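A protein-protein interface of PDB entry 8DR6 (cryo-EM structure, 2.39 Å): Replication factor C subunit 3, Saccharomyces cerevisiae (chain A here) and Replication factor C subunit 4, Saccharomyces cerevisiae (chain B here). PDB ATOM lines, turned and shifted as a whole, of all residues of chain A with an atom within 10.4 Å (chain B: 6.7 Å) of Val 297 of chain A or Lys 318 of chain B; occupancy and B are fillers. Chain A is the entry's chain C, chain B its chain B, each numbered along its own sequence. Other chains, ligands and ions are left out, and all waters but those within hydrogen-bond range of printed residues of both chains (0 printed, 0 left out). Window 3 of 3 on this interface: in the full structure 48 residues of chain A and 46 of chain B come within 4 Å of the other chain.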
ATOM      1  N   LEU A 285       8.923 -20.667 -14.251  1.00  0.00           N
ATOM      2  CA  LEU A 285       8.505 -20.387 -12.883  1.00  0.00           C
ATOM      3  C   LEU A 285       6.992 -20.326 -12.737  1.00  0.00           C
ATOM      4  O   LEU A 285       6.482 -20.515 -11.628  1.00  0.00           O
ATOM      5  CB  LEU A 285       9.120 -19.070 -12.406  1.00  0.00           C
ATOM      6  CG  LEU A 285      10.621 -19.087 -12.105  1.00  0.00           C
ATOM      7  CD1 LEU A 285      11.111 -17.687 -11.770  1.00  0.00           C
ATOM      8  CD2 LEU A 285      10.945 -20.050 -10.972  1.00  0.00           C
ATOM      9  N   LEU A 290       4.649 -22.359  -5.083  1.00  0.00           N
ATOM     10  CA  LEU A 290       5.313 -21.549  -4.072  1.00  0.00           C
ATOM     11  C   LEU A 290       4.457 -21.465  -2.815  1.00  0.00           C
ATOM     12  O   LEU A 290       3.225 -21.465  -2.878  1.00  0.00           O
ATOM     13  CB  LEU A 290       5.600 -20.141  -4.601  1.00  0.00           C
ATOM     14  CG  LEU A 290       6.353 -20.080  -5.933  1.00  0.00           C
ATOM     15  CD1 LEU A 290       6.302 -18.677  -6.517  1.00  0.00           C
ATOM     16  CD2 LEU A 290       7.792 -20.541  -5.759  1.00  0.00           C
ATOM     17  N   GLN A 291       5.132 -21.393  -1.667  1.00  0.00           N
ATOM     18  CA  GLN A 291       4.424 -21.371  -0.389  1.00  0.00           C
ATOM     19  C   GLN A 291       3.846 -19.992  -0.091  1.00  0.00           C
ATOM     20  O   GLN A 291       2.775 -19.887   0.516  1.00  0.00           O
ATOM     21  CB  GLN A 291       5.341 -21.812   0.761  1.00  0.00           C
ATOM     22  CG  GLN A 291       6.583 -22.636   0.392  1.00  0.00           C
ATOM     23  CD  GLN A 291       6.277 -24.110   0.213  1.00  0.00           C
ATOM     24  OE1 GLN A 291       5.263 -24.611   0.700  1.00  0.00           O
ATOM     25  NE2 GLN A 291       7.156 -24.815  -0.490  1.00  0.00           N
ATOM     26  N   ASN A 292       4.534 -18.931  -0.506  1.00  0.00           N
ATOM     27  CA  ASN A 292       4.153 -17.565  -0.177  1.00  0.00           C
ATOM     28  C   ASN A 292       3.807 -16.789  -1.440  1.00  0.00           C
ATOM     29  O   ASN A 292       4.488 -16.909  -2.462  1.00  0.00           O
ATOM     30  CB  ASN A 292       5.282 -16.855   0.575  1.00  0.00           C
ATOM     31  CG  ASN A 292       4.789 -15.672   1.386  1.00  0.00           C
ATOM     32  OD1 ASN A 292       3.615 -15.306   1.324  1.00  0.00           O
ATOM     33  ND2 ASN A 292       5.688 -15.067   2.154  1.00  0.00           N
ATOM     34  N   GLU A 293       2.739 -15.991  -1.359  1.00  0.00           N
ATOM     35  CA  GLU A 293       2.352 -15.133  -2.473  1.00  0.00           C
ATOM     36  C   GLU A 293       3.319 -13.972  -2.666  1.00  0.00           C
ATOM     37  O   GLU A 293       3.392 -13.416  -3.769  1.00  0.00           O
ATOM     38  CB  GLU A 293       0.938 -14.595  -2.252  1.00  0.00           C
ATOM     39  CG  GLU A 293      -0.005 -14.823  -3.420  1.00  0.00           C
ATOM     40  CD  GLU A 293      -1.361 -14.179  -3.205  1.00  0.00           C
ATOM     41  OE1 GLU A 293      -1.433 -12.932  -3.185  1.00  0.00           O
ATOM     42  OE2 GLU A 293      -2.356 -14.920  -3.054  1.00  0.00           O
ATOM     43  N   GLU A 294       4.057 -13.593  -1.619  1.00  0.00           N
ATOM     44  CA  GLU A 294       5.017 -12.503  -1.747  1.00  0.00           C
ATOM     45  C   GLU A 294       6.086 -12.837  -2.777  1.00  0.00           C
ATOM     46  O   GLU A 294       6.538 -11.959  -3.520  1.00  0.00           O
ATOM     47  CB  GLU A 294       5.659 -12.209  -0.389  1.00  0.00           C
ATOM     48  CG  GLU A 294       4.754 -11.506   0.625  1.00  0.00           C
ATOM     49  CD  GLU A 294       3.876 -10.433   0.009  1.00  0.00           C
ATOM     50  OE1 GLU A 294       2.809 -10.780  -0.540  1.00  0.00           O
ATOM     51  OE2 GLU A 294       4.251  -9.244   0.075  1.00  0.00           O
ATOM     52  N   THR A 295       6.510 -14.101  -2.830  1.00  0.00           N
ATOM     53  CA  THR A 295       7.483 -14.517  -3.834  1.00  0.00           C
ATOM     54  C   THR A 295       6.965 -14.236  -5.239  1.00  0.00           C
ATOM     55  O   THR A 295       7.663 -13.634  -6.064  1.00  0.00           O
ATOM     56  CB  THR A 295       7.800 -16.004  -3.669  1.00  0.00           C
ATOM     57  OG1 THR A 295       8.173 -16.271  -2.311  1.00  0.00           O
ATOM     58  CG2 THR A 295       8.931 -16.421  -4.601  1.00  0.00           C
ATOM     59  N   ARG A 296       5.735 -14.668  -5.526  1.00  0.00           N
ATOM     60  CA  ARG A 296       5.162 -14.446  -6.848  1.00  0.00           C
ATOM     61  C   ARG A 296       5.018 -12.959  -7.142  1.00  0.00           C
ATOM     62  O   ARG A 296       5.329 -12.506  -8.251  1.00  0.00           O
ATOM     63  CB  ARG A 296       3.807 -15.150  -6.952  1.00  0.00           C
ATOM     64  CG  ARG A 296       3.096 -14.979  -8.294  1.00  0.00           C
ATOM     65  CD  ARG A 296       3.488 -16.062  -9.285  1.00  0.00           C
ATOM     66  NE  ARG A 296       3.048 -17.385  -8.855  1.00  0.00           N
ATOM     67  CZ  ARG A 296       3.666 -18.521  -9.150  1.00  0.00           C
ATOM     68  NH1 ARG A 296       4.761 -18.542  -9.895  1.00  0.00           N
ATOM     69  NH2 ARG A 296       3.172 -19.667  -8.689  1.00  0.00           N
ATOM     70  N   VAL A 297       4.545 -12.183  -6.165  1.00  0.00           N
ATOM     71  CA  VAL A 297       4.356 -10.753  -6.390  1.00  0.00           C
ATOM     72  C   VAL A 297       5.685 -10.086  -6.721  1.00  0.00           C
ATOM     73  O   VAL A 297       5.793  -9.333  -7.700  1.00  0.00           O
ATOM     74  CB  VAL A 297       3.691 -10.107  -5.161  1.00  0.00           C
ATOM     75  CG1 VAL A 297       3.788  -8.589  -5.234  1.00  0.00           C
ATOM     76  CG2 VAL A 297       2.240 -10.548  -5.049  1.00  0.00           C
ATOM     77  N   HIS A 298       6.716 -10.348  -5.915  1.00  0.00           N
ATOM     78  CA  HIS A 298       8.020  -9.741  -6.153  1.00  0.00           C
ATOM     79  C   HIS A 298       8.581 -10.166  -7.502  1.00  0.00           C
ATOM     80  O   HIS A 298       9.068  -9.329  -8.274  1.00  0.00           O
ATOM     81  CB  HIS A 298       8.985 -10.121  -5.028  1.00  0.00           C
ATOM     82  CG  HIS A 298       8.879  -9.245  -3.818  1.00  0.00           C
ATOM     83  ND1 HIS A 298       7.752  -9.205  -3.025  1.00  0.00           N
ATOM     84  CD2 HIS A 298       9.760  -8.379  -3.266  1.00  0.00           C
ATOM     85  CE1 HIS A 298       7.944  -8.351  -2.037  1.00  0.00           C
ATOM     86  NE2 HIS A 298       9.154  -7.835  -2.159  1.00  0.00           N
ATOM     87  N   LEU A 299       8.519 -11.464  -7.808  1.00  0.00           N
ATOM     88  CA  LEU A 299       9.034 -11.943  -9.084  1.00  0.00           C
ATOM     89  C   LEU A 299       8.350 -11.234 -10.243  1.00  0.00           C
ATOM     90  O   LEU A 299       9.014 -10.681 -11.128  1.00  0.00           O
ATOM     91  CB  LEU A 299       8.839 -13.456  -9.195  1.00  0.00           C
ATOM     92  CG  LEU A 299       9.977 -14.338  -8.680  1.00  0.00           C
ATOM     93  CD1 LEU A 299       9.518 -15.783  -8.563  1.00  0.00           C
ATOM     94  CD2 LEU A 299      11.198 -14.233  -9.583  1.00  0.00           C
ATOM     95  N   LEU A 300       7.016 -11.225 -10.246  1.00  0.00           N
ATOM     96  CA  LEU A 300       6.286 -10.631 -11.359  1.00  0.00           C
ATOM     97  C   LEU A 300       6.608  -9.149 -11.496  1.00  0.00           C
ATOM     98  O   LEU A 300       6.937  -8.678 -12.591  1.00  0.00           O
ATOM     99  CB  LEU A 300       4.783 -10.842 -11.172  1.00  0.00           C
ATOM    100  CG  LEU A 300       4.298 -12.289 -11.283  1.00  0.00           C
ATOM    101  CD1 LEU A 300       2.845 -12.398 -10.850  1.00  0.00           C
ATOM    102  CD2 LEU A 300       4.478 -12.816 -12.698  1.00  0.00           C
ATOM    103  N   THR A 301       6.539  -8.398 -10.393  1.00  0.00           N
ATOM    104  CA  THR A 301       6.760  -6.958 -10.482  1.00  0.00           C
ATOM    105  C   THR A 301       8.175  -6.641 -10.954  1.00  0.00           C
ATOM    106  O   THR A 301       8.365  -5.842 -11.880  1.00  0.00           O
ATOM    107  CB  THR A 301       6.489  -6.299  -9.129  1.00  0.00           C
ATOM    108  OG1 THR A 301       7.320  -6.896  -8.125  1.00  0.00           O
ATOM    109  CG2 THR A 301       5.025  -6.454  -8.739  1.00  0.00           C
ATOM    110  N   LYS A 302       9.182  -7.261 -10.335  1.00  0.00           N
ATOM    111  CA  LYS A 302      10.562  -6.948 -10.683  1.00  0.00           C
ATOM    112  C   LYS A 302      10.894  -7.381 -12.107  1.00  0.00           C
ATOM    113  O   LYS A 302      11.578  -6.650 -12.833  1.00  0.00           O
ATOM    114  CB  LYS A 302      11.510  -7.603  -9.678  1.00  0.00           C
ATOM    115  CG  LYS A 302      11.387  -7.023  -8.275  1.00  0.00           C
ATOM    116  CD  LYS A 302      12.392  -7.631  -7.312  1.00  0.00           C
ATOM    117  CE  LYS A 302      13.597  -6.725  -7.126  1.00  0.00           C
ATOM    118  NZ  LYS A 302      13.288  -5.554  -6.259  1.00  0.00           N
ATOM    119  N   LEU A 303      10.418  -8.553 -12.534  1.00  0.00           N
ATOM    120  CA  LEU A 303      10.696  -8.997 -13.894  1.00  0.00           C
ATOM    121  C   LEU A 303       9.979  -8.133 -14.923  1.00  0.00           C
ATOM    122  O   LEU A 303      10.539  -7.858 -15.989  1.00  0.00           O
ATOM    123  CB  LEU A 303      10.304 -10.466 -14.052  1.00  0.00           C
ATOM    124  CG  LEU A 303      11.170 -11.447 -13.254  1.00  0.00           C
ATOM    125  CD1 LEU A 303      10.614 -12.857 -13.340  1.00  0.00           C
ATOM    126  CD2 LEU A 303      12.616 -11.415 -13.731  1.00  0.00           C
ATOM    127  N   ALA A 304       8.753  -7.690 -14.631  1.00  0.00           N
ATOM    128  CA  ALA A 304       8.075  -6.770 -15.537  1.00  0.00           C
ATOM    129  C   ALA A 304       8.830  -5.452 -15.643  1.00  0.00           C
ATOM    130  O   ALA A 304       8.974  -4.897 -16.739  1.00  0.00           O
ATOM    131  CB  ALA A 304       6.641  -6.532 -15.068  1.00  0.00           C
ATOM    132  N   ASP A 305       9.324  -4.936 -14.513  1.00  0.00           N
ATOM    133  CA  ASP A 305      10.110  -3.707 -14.554  1.00  0.00           C
ATOM    134  C   ASP A 305      11.381  -3.897 -15.374  1.00  0.00           C
ATOM    135  O   ASP A 305      11.760  -3.019 -16.158  1.00  0.00           O
ATOM    136  CB  ASP A 305      10.451  -3.257 -13.134  1.00  0.00           C
ATOM    137  CG  ASP A 305       9.347  -2.432 -12.504  1.00  0.00           C
ATOM    138  OD1 ASP A 305       8.181  -2.873 -12.537  1.00  0.00           O
ATOM    139  OD2 ASP A 305       9.648  -1.340 -11.976  1.00  0.00           O
ATOM    140  N   ALA A 326      16.964 -10.070  -8.371  1.00  0.00           N
ATOM    141  CA  ALA A 326      15.527 -10.095  -8.141  1.00  0.00           C
ATOM    142  C   ALA A 326      15.041 -11.510  -7.873  1.00  0.00           C
ATOM    143  O   ALA A 326      14.262 -11.736  -6.940  1.00  0.00           O
ATOM    144  CB  ALA A 326      14.795  -9.495  -9.340  1.00  0.00           C
ATOM    145  N   ILE A 327      15.493 -12.479  -8.671  1.00  0.00           N
ATOM    146  CA  ILE A 327      15.078 -13.861  -8.444  1.00  0.00           C
ATOM    147  C   ILE A 327      15.557 -14.338  -7.078  1.00  0.00           C
ATOM    148  O   ILE A 327      14.799 -14.950  -6.312  1.00  0.00           O
ATOM    149  CB  ILE A 327      15.592 -14.769  -9.574  1.00  0.00           C
ATOM    150  CG1 ILE A 327      14.880 -14.428 -10.887  1.00  0.00           C
ATOM    151  CG2 ILE A 327      15.384 -16.237  -9.212  1.00  0.00           C
ATOM    152  CD1 ILE A 327      15.443 -15.136 -12.102  1.00  0.00           C
ATOM    153  N   ALA A 329      16.325 -12.606  -4.360  1.00  0.00           N
ATOM    154  CA  ALA A 329      15.623 -11.949  -3.263  1.00  0.00           C
ATOM    155  C   ALA A 329      14.182 -12.431  -3.160  1.00  0.00           C
ATOM    156  O   ALA A 329      13.663 -12.620  -2.054  1.00  0.00           O
ATOM    157  CB  ALA A 329      15.668 -10.433  -3.447  1.00  0.00           C
ATOM    158  N   SER A 330      13.515 -12.632  -4.300  1.00  0.00           N
ATOM    159  CA  SER A 330      12.135 -13.098  -4.270  1.00  0.00           C
ATOM    160  C   SER A 330      12.039 -14.494  -3.673  1.00  0.00           C
ATOM    161  O   SER A 330      11.120 -14.780  -2.896  1.00  0.00           O
ATOM    162  CB  SER A 330      11.546 -13.077  -5.680  1.00  0.00           C
ATOM    163  OG  SER A 330      11.866 -11.869  -6.347  1.00  0.00           O
ATOM    164  N   PHE A 331      12.978 -15.376  -4.013  1.00  0.00           N
ATOM    165  CA  PHE A 331      12.938 -16.736  -3.489  1.00  0.00           C
ATOM    166  C   PHE A 331      13.348 -16.825  -2.025  1.00  0.00           C
ATOM    167  O   PHE A 331      13.233 -17.903  -1.433  1.00  0.00           O
ATOM    168  CB  PHE A 331      13.822 -17.652  -4.335  1.00  0.00           C
ATOM    169  CG  PHE A 331      13.068 -18.401  -5.396  1.00  0.00           C
ATOM    170  CD1 PHE A 331      12.803 -17.816  -6.623  1.00  0.00           C
ATOM    171  CD2 PHE A 331      12.614 -19.689  -5.163  1.00  0.00           C
ATOM    172  CE1 PHE A 331      12.104 -18.501  -7.598  1.00  0.00           C
ATOM    173  CE2 PHE A 331      11.915 -20.380  -6.134  1.00  0.00           C
ATOM    174  CZ  PHE A 331      11.660 -19.784  -7.353  1.00  0.00           C
ATOM    175  N   ASN A 333      11.724 -15.364   0.309  1.00  0.00           N
ATOM    176  CA  ASN A 333      10.480 -15.326   1.067  1.00  0.00           C
ATOM    177  C   ASN A 333       9.853 -16.701   1.243  1.00  0.00           C
ATOM    178  O   ASN A 333       8.844 -16.817   1.946  1.00  0.00           O
ATOM    179  CB  ASN A 333       9.476 -14.393   0.381  1.00  0.00           C
ATOM    180  CG  ASN A 333      10.068 -13.034   0.051  1.00  0.00           C
ATOM    181  OD1 ASN A 333       9.738 -12.436  -0.974  1.00  0.00           O
ATOM    182  ND2 ASN A 333      10.938 -12.535   0.921  1.00  0.00           N
ATOM    183  N   GLU A 334      10.418 -17.739   0.629  1.00  0.00           N
ATOM    184  CA  GLU A 334       9.882 -19.089   0.736  1.00  0.00           C
ATOM    185  C   GLU A 334      10.305 -19.799   2.014  1.00  0.00           C
ATOM    186  O   GLU A 334       9.807 -20.895   2.289  1.00  0.00           O
ATOM    187  CB  GLU A 334      10.319 -19.925  -0.471  1.00  0.00           C
ATOM    188  CG  GLU A 334       9.673 -19.508  -1.781  1.00  0.00           C
ATOM    189  CD  GLU A 334       8.196 -19.842  -1.837  1.00  0.00           C
ATOM    190  OE1 GLU A 334       7.381 -19.015  -1.380  1.00  0.00           O
ATOM    191  OE2 GLU A 334       7.851 -20.933  -2.337  1.00  0.00           O
ATOM    192  N   LEU B 245      -4.059 -14.255  -5.460  1.00  0.00           N
ATOM    193  CA  LEU B 245      -3.403 -13.866  -6.703  1.00  0.00           C
ATOM    194  C   LEU B 245      -3.387 -15.019  -7.698  1.00  0.00           C
ATOM    195  O   LEU B 245      -3.479 -14.801  -8.913  1.00  0.00           O
ATOM    196  CB  LEU B 245      -1.981 -13.385  -6.415  1.00  0.00           C
ATOM    197  CG  LEU B 245      -1.115 -13.039  -7.629  1.00  0.00           C
ATOM    198  CD1 LEU B 245      -1.805 -12.014  -8.518  1.00  0.00           C
ATOM    199  CD2 LEU B 245       0.246 -12.532  -7.183  1.00  0.00           C
ATOM    200  N   GLU B 291      -2.576   1.985 -10.881  1.00  0.00           N
ATOM    201  CA  GLU B 291      -1.791   0.844 -11.349  1.00  0.00           C
ATOM    202  C   GLU B 291      -2.199   0.431 -12.761  1.00  0.00           C
ATOM    203  O   GLU B 291      -1.341   0.145 -13.608  1.00  0.00           O
ATOM    204  CB  GLU B 291      -1.944  -0.332 -10.382  1.00  0.00           C
ATOM    205  CG  GLU B 291      -1.509  -0.035  -8.952  1.00  0.00           C
ATOM    206  CD  GLU B 291      -0.004   0.107  -8.805  1.00  0.00           C
ATOM    207  OE1 GLU B 291       0.687   0.289  -9.828  1.00  0.00           O
ATOM    208  OE2 GLU B 291       0.488   0.036  -7.660  1.00  0.00           O
ATOM    209  N   SER B 311       1.947  -8.682 -13.620  1.00  0.00           N
ATOM    210  CA  SER B 311       2.469  -7.711 -12.664  1.00  0.00           C
ATOM    211  C   SER B 311       1.379  -6.748 -12.208  1.00  0.00           C
ATOM    212  O   SER B 311       1.330  -6.370 -11.033  1.00  0.00           O
ATOM    213  CB  SER B 311       3.635  -6.942 -13.283  1.00  0.00           C
ATOM    214  OG  SER B 311       4.106  -5.936 -12.403  1.00  0.00           O
ATOM    215  N   LEU B 313      -1.831  -7.430 -11.987  1.00  0.00           N
ATOM    216  CA  LEU B 313      -2.660  -8.178 -11.046  1.00  0.00           C
ATOM    217  C   LEU B 313      -1.967  -8.321  -9.696  1.00  0.00           C
ATOM    218  O   LEU B 313      -2.607  -8.199  -8.644  1.00  0.00           O
ATOM    219  CB  LEU B 313      -2.997  -9.553 -11.623  1.00  0.00           C
ATOM    220  CG  LEU B 313      -3.992  -9.584 -12.787  1.00  0.00           C
ATOM    221  CD1 LEU B 313      -4.214 -11.013 -13.252  1.00  0.00           C
ATOM    222  CD2 LEU B 313      -5.314  -8.937 -12.400  1.00  0.00           C
ATOM    223  N   ALA B 314      -0.659  -8.588  -9.706  1.00  0.00           N
ATOM    224  CA  ALA B 314       0.080  -8.714  -8.455  1.00  0.00           C
ATOM    225  C   ALA B 314       0.058  -7.409  -7.670  1.00  0.00           C
ATOM    226  O   ALA B 314      -0.126  -7.413  -6.449  1.00  0.00           O
ATOM    227  CB  ALA B 314       1.518  -9.147  -8.737  1.00  0.00           C
ATOM    228  N   LYS B 315       0.249  -6.279  -8.355  1.00  0.00           N
ATOM    229  CA  LYS B 315       0.188  -4.986  -7.682  1.00  0.00           C
ATOM    230  C   LYS B 315      -1.203  -4.710  -7.129  1.00  0.00           C
ATOM    231  O   LYS B 315      -1.335  -4.194  -6.012  1.00  0.00           O
ATOM    232  CB  LYS B 315       0.605  -3.874  -8.643  1.00  0.00           C
ATOM    233  CG  LYS B 315       2.095  -3.841  -8.940  1.00  0.00           C
ATOM    234  CD  LYS B 315       2.484  -2.579  -9.693  1.00  0.00           C
ATOM    235  CE  LYS B 315       3.909  -2.657 -10.212  1.00  0.00           C
ATOM    236  NZ  LYS B 315       4.230  -1.534 -11.134  1.00  0.00           N
ATOM    237  N   ILE B 316      -2.249  -5.044  -7.889  1.00  0.00           N
ATOM    238  CA  ILE B 316      -3.609  -4.849  -7.396  1.00  0.00           C
ATOM    239  C   ILE B 316      -3.837  -5.669  -6.133  1.00  0.00           C
ATOM    240  O   ILE B 316      -4.412  -5.179  -5.154  1.00  0.00           O
ATOM    241  CB  ILE B 316      -4.630  -5.198  -8.494  1.00  0.00           C
ATOM    242  CG1 ILE B 316      -4.661  -4.097  -9.556  1.00  0.00           C
ATOM    243  CG2 ILE B 316      -6.015  -5.401  -7.887  1.00  0.00           C
ATOM    244  CD1 ILE B 316      -5.421  -4.472 -10.813  1.00  0.00           C
ATOM    245  N   HIS B 317      -3.394  -6.927  -6.134  1.00  0.00           N
ATOM    246  CA  HIS B 317      -3.550  -7.761  -4.946  1.00  0.00           C
ATOM    247  C   HIS B 317      -2.751  -7.205  -3.774  1.00  0.00           C
ATOM    248  O   HIS B 317      -3.221  -7.226  -2.630  1.00  0.00           O
ATOM    249  CB  HIS B 317      -3.131  -9.198  -5.253  1.00  0.00           C
ATOM    250  CG  HIS B 317      -4.274 -10.089  -5.627  1.00  0.00           C
ATOM    251  ND1 HIS B 317      -4.715 -10.230  -6.925  1.00  0.00           N
ATOM    252  CD2 HIS B 317      -5.070 -10.881  -4.870  1.00  0.00           C
ATOM    253  CE1 HIS B 317      -5.732 -11.073  -6.952  1.00  0.00           C
ATOM    254  NE2 HIS B 317      -5.968 -11.483  -5.719  1.00  0.00           N
ATOM    255  N   LYS B 318      -1.541  -6.705  -4.035  1.00  0.00           N
ATOM    256  CA  LYS B 318      -0.741  -6.109  -2.971  1.00  0.00           C
ATOM    257  C   LYS B 318      -1.426  -4.886  -2.380  1.00  0.00           C
ATOM    258  O   LYS B 318      -1.314  -4.634  -1.175  1.00  0.00           O
ATOM    259  CB  LYS B 318       0.643  -5.735  -3.502  1.00  0.00           C
ATOM    260  CG  LYS B 318       1.651  -5.392  -2.415  1.00  0.00           C
ATOM    261  CD  LYS B 318       3.089  -5.521  -2.900  1.00  0.00           C
ATOM    262  CE  LYS B 318       3.344  -4.723  -4.173  1.00  0.00           C
ATOM    263  NZ  LYS B 318       4.746  -4.874  -4.651  1.00  0.00           N
ATOM    264  N   LEU B 319      -2.135  -4.114  -3.207  1.00  0.00           N
ATOM    265  CA  LEU B 319      -2.837  -2.941  -2.698  1.00  0.00           C
ATOM    266  C   LEU B 319      -3.898  -3.333  -1.676  1.00  0.00           C
ATOM    267  O   LEU B 319      -4.093  -2.631  -0.677  1.00  0.00           O
ATOM    268  CB  LEU B 319      -3.471  -2.164  -3.850  1.00  0.00           C
ATOM    269  CG  LEU B 319      -2.536  -1.245  -4.637  1.00  0.00           C
ATOM    270  CD1 LEU B 319      -3.188  -0.815  -5.940  1.00  0.00           C
ATOM    271  CD2 LEU B 319      -2.145  -0.032  -3.805  1.00  0.00           C
ATOM    272  N   ASN B 320      -4.592  -4.445  -1.907  1.00  0.00           N
ATOM    273  CA  ASN B 320      -5.664  -4.894  -1.031  1.00  0.00           C
ATOM    274  C   ASN B 320      -5.156  -5.684   0.169  1.00  0.00           C
ATOM    275  O   ASN B 320      -5.964  -6.104   1.004  1.00  0.00           O
ATOM    276  CB  ASN B 320      -6.662  -5.744  -1.820  1.00  0.00           C
ATOM    277  CG  ASN B 320      -7.468  -4.928  -2.811  1.00  0.00           C
ATOM    278  OD1 ASN B 320      -8.497  -4.347  -2.464  1.00  0.00           O
ATOM    279  ND2 ASN B 320      -7.004  -4.880  -4.054  1.00  0.00           N
ATOM    280  N   ASN B 321      -3.848  -5.893   0.276  1.00  0.00           N
ATOM    281  CA  ASN B 321      -3.277  -6.624   1.402  1.00  0.00           C
ATOM    282  C   ASN B 321      -2.695  -5.662   2.432  1.00  0.00           C
ATOM    283  O   ASN B 321      -1.540  -5.251   2.328  1.00  0.00           O
ATOM    284  CB  ASN B 321      -2.196  -7.593   0.919  1.00  0.00           C
ATOM    285  CG  ASN B 321      -2.761  -8.732   0.094  1.00  0.00           C
ATOM    286  OD1 ASN B 321      -3.969  -8.973   0.091  1.00  0.00           O
ATOM    287  ND2 ASN B 321      -1.889  -9.442  -0.613  1.00  0.00           N
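The side-chain carboxylate (OE2) of Glu 293 of chain A lies within hydrogen-bond range of the backbone NH (N) of Leu 245 of chain B, 3.0 Å away.
OG1 of Thr 301 of chain A is in hydrogen-bond range of O of Val 297 of chain A, at 2.9 Å.
N of Leu 245 of chain B sits at hydrogen-bond distance from NE2 of His 317 of chain B, 3.4 Å away.
The backbone carbonyl oxygen (O) of His 298 of chain A lies within hydrogen-bond range of the side-chain hydroxyl (OG1) of Thr 301 of chain A, at 3.0 Å.
NH1 of Arg 296 of chain A sits at hydrogen-bond distance from O of Leu 285 of chain A (3.1 Å).
CG of Arg 296 of chain A touches CD2 of Leu 245 of chain B (3.9 Å).
Leu 245 of chain B touches Val 297 of chain A (CD2 to CG2, 3.5 Å).
CG1 of Val 297 of chain A touches NZ of Lys 318 of chain B, at 3.9 Å.
Leu 300 of chain A touches Ser 311 of chain B.
Ser 311 of chain B touches Thr 301 of chain A (OG to CA, 3.4 Å).
Thr 301 of chain A touches Lys 315 of chain B (CG2 to CG, 3.9 Å).
CB of Ala 304 of chain A touches CB of Ser 311 of chain B, 3.5 Å away.
Printed residues of chain B within 4 Å of Val 297 of chain A: Leu 245 and Lys 318.
Printed residues of chain B within 4 Å of Leu 300 of chain A: Ser 311 (3.8 Å).
Of the printed residues of chain B, Thr 301 of chain A touches Ser 311 and Lys 315.
Leu 303 of chain A touches none of the printed residues of chain B.
Asp 305 of chain A touches none of the printed residues of chain B.
Printed residues of chain A within 4 Å of Ser 311 of chain B: Leu 300, Thr 301 and Ala 304.
Lys 318 of chain B touches one residue of chain A.
No residue of chain A comes within 4 Å of Leu 319 of chain B.
Asn 321 of chain B touches none of the printed residues of chain A.
The nearest printed residue of chain A that does not touch Leu 245 of chain B is Leu 300 of chain A (4.5 Å).
Of the 24 printed residues of chain A, 6 touch a printed residue of chain B.
Of the 12 printed residues of chain B, 4 touch a printed residue of chain A.
Hydrophobic or aromatic side chains of chain B within 4 Å of the printed part of chain A: Leu 245.
Along chain B the printed residues that touch a printed residue of chain A span positions 245 to 318.
Among the printed residues, 8 pairs touch across the chains.
Among the printed residues, no Asp or Glu carboxylate lies within 4 Å of a Lys or Arg side-chain nitrogen of the other chain.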
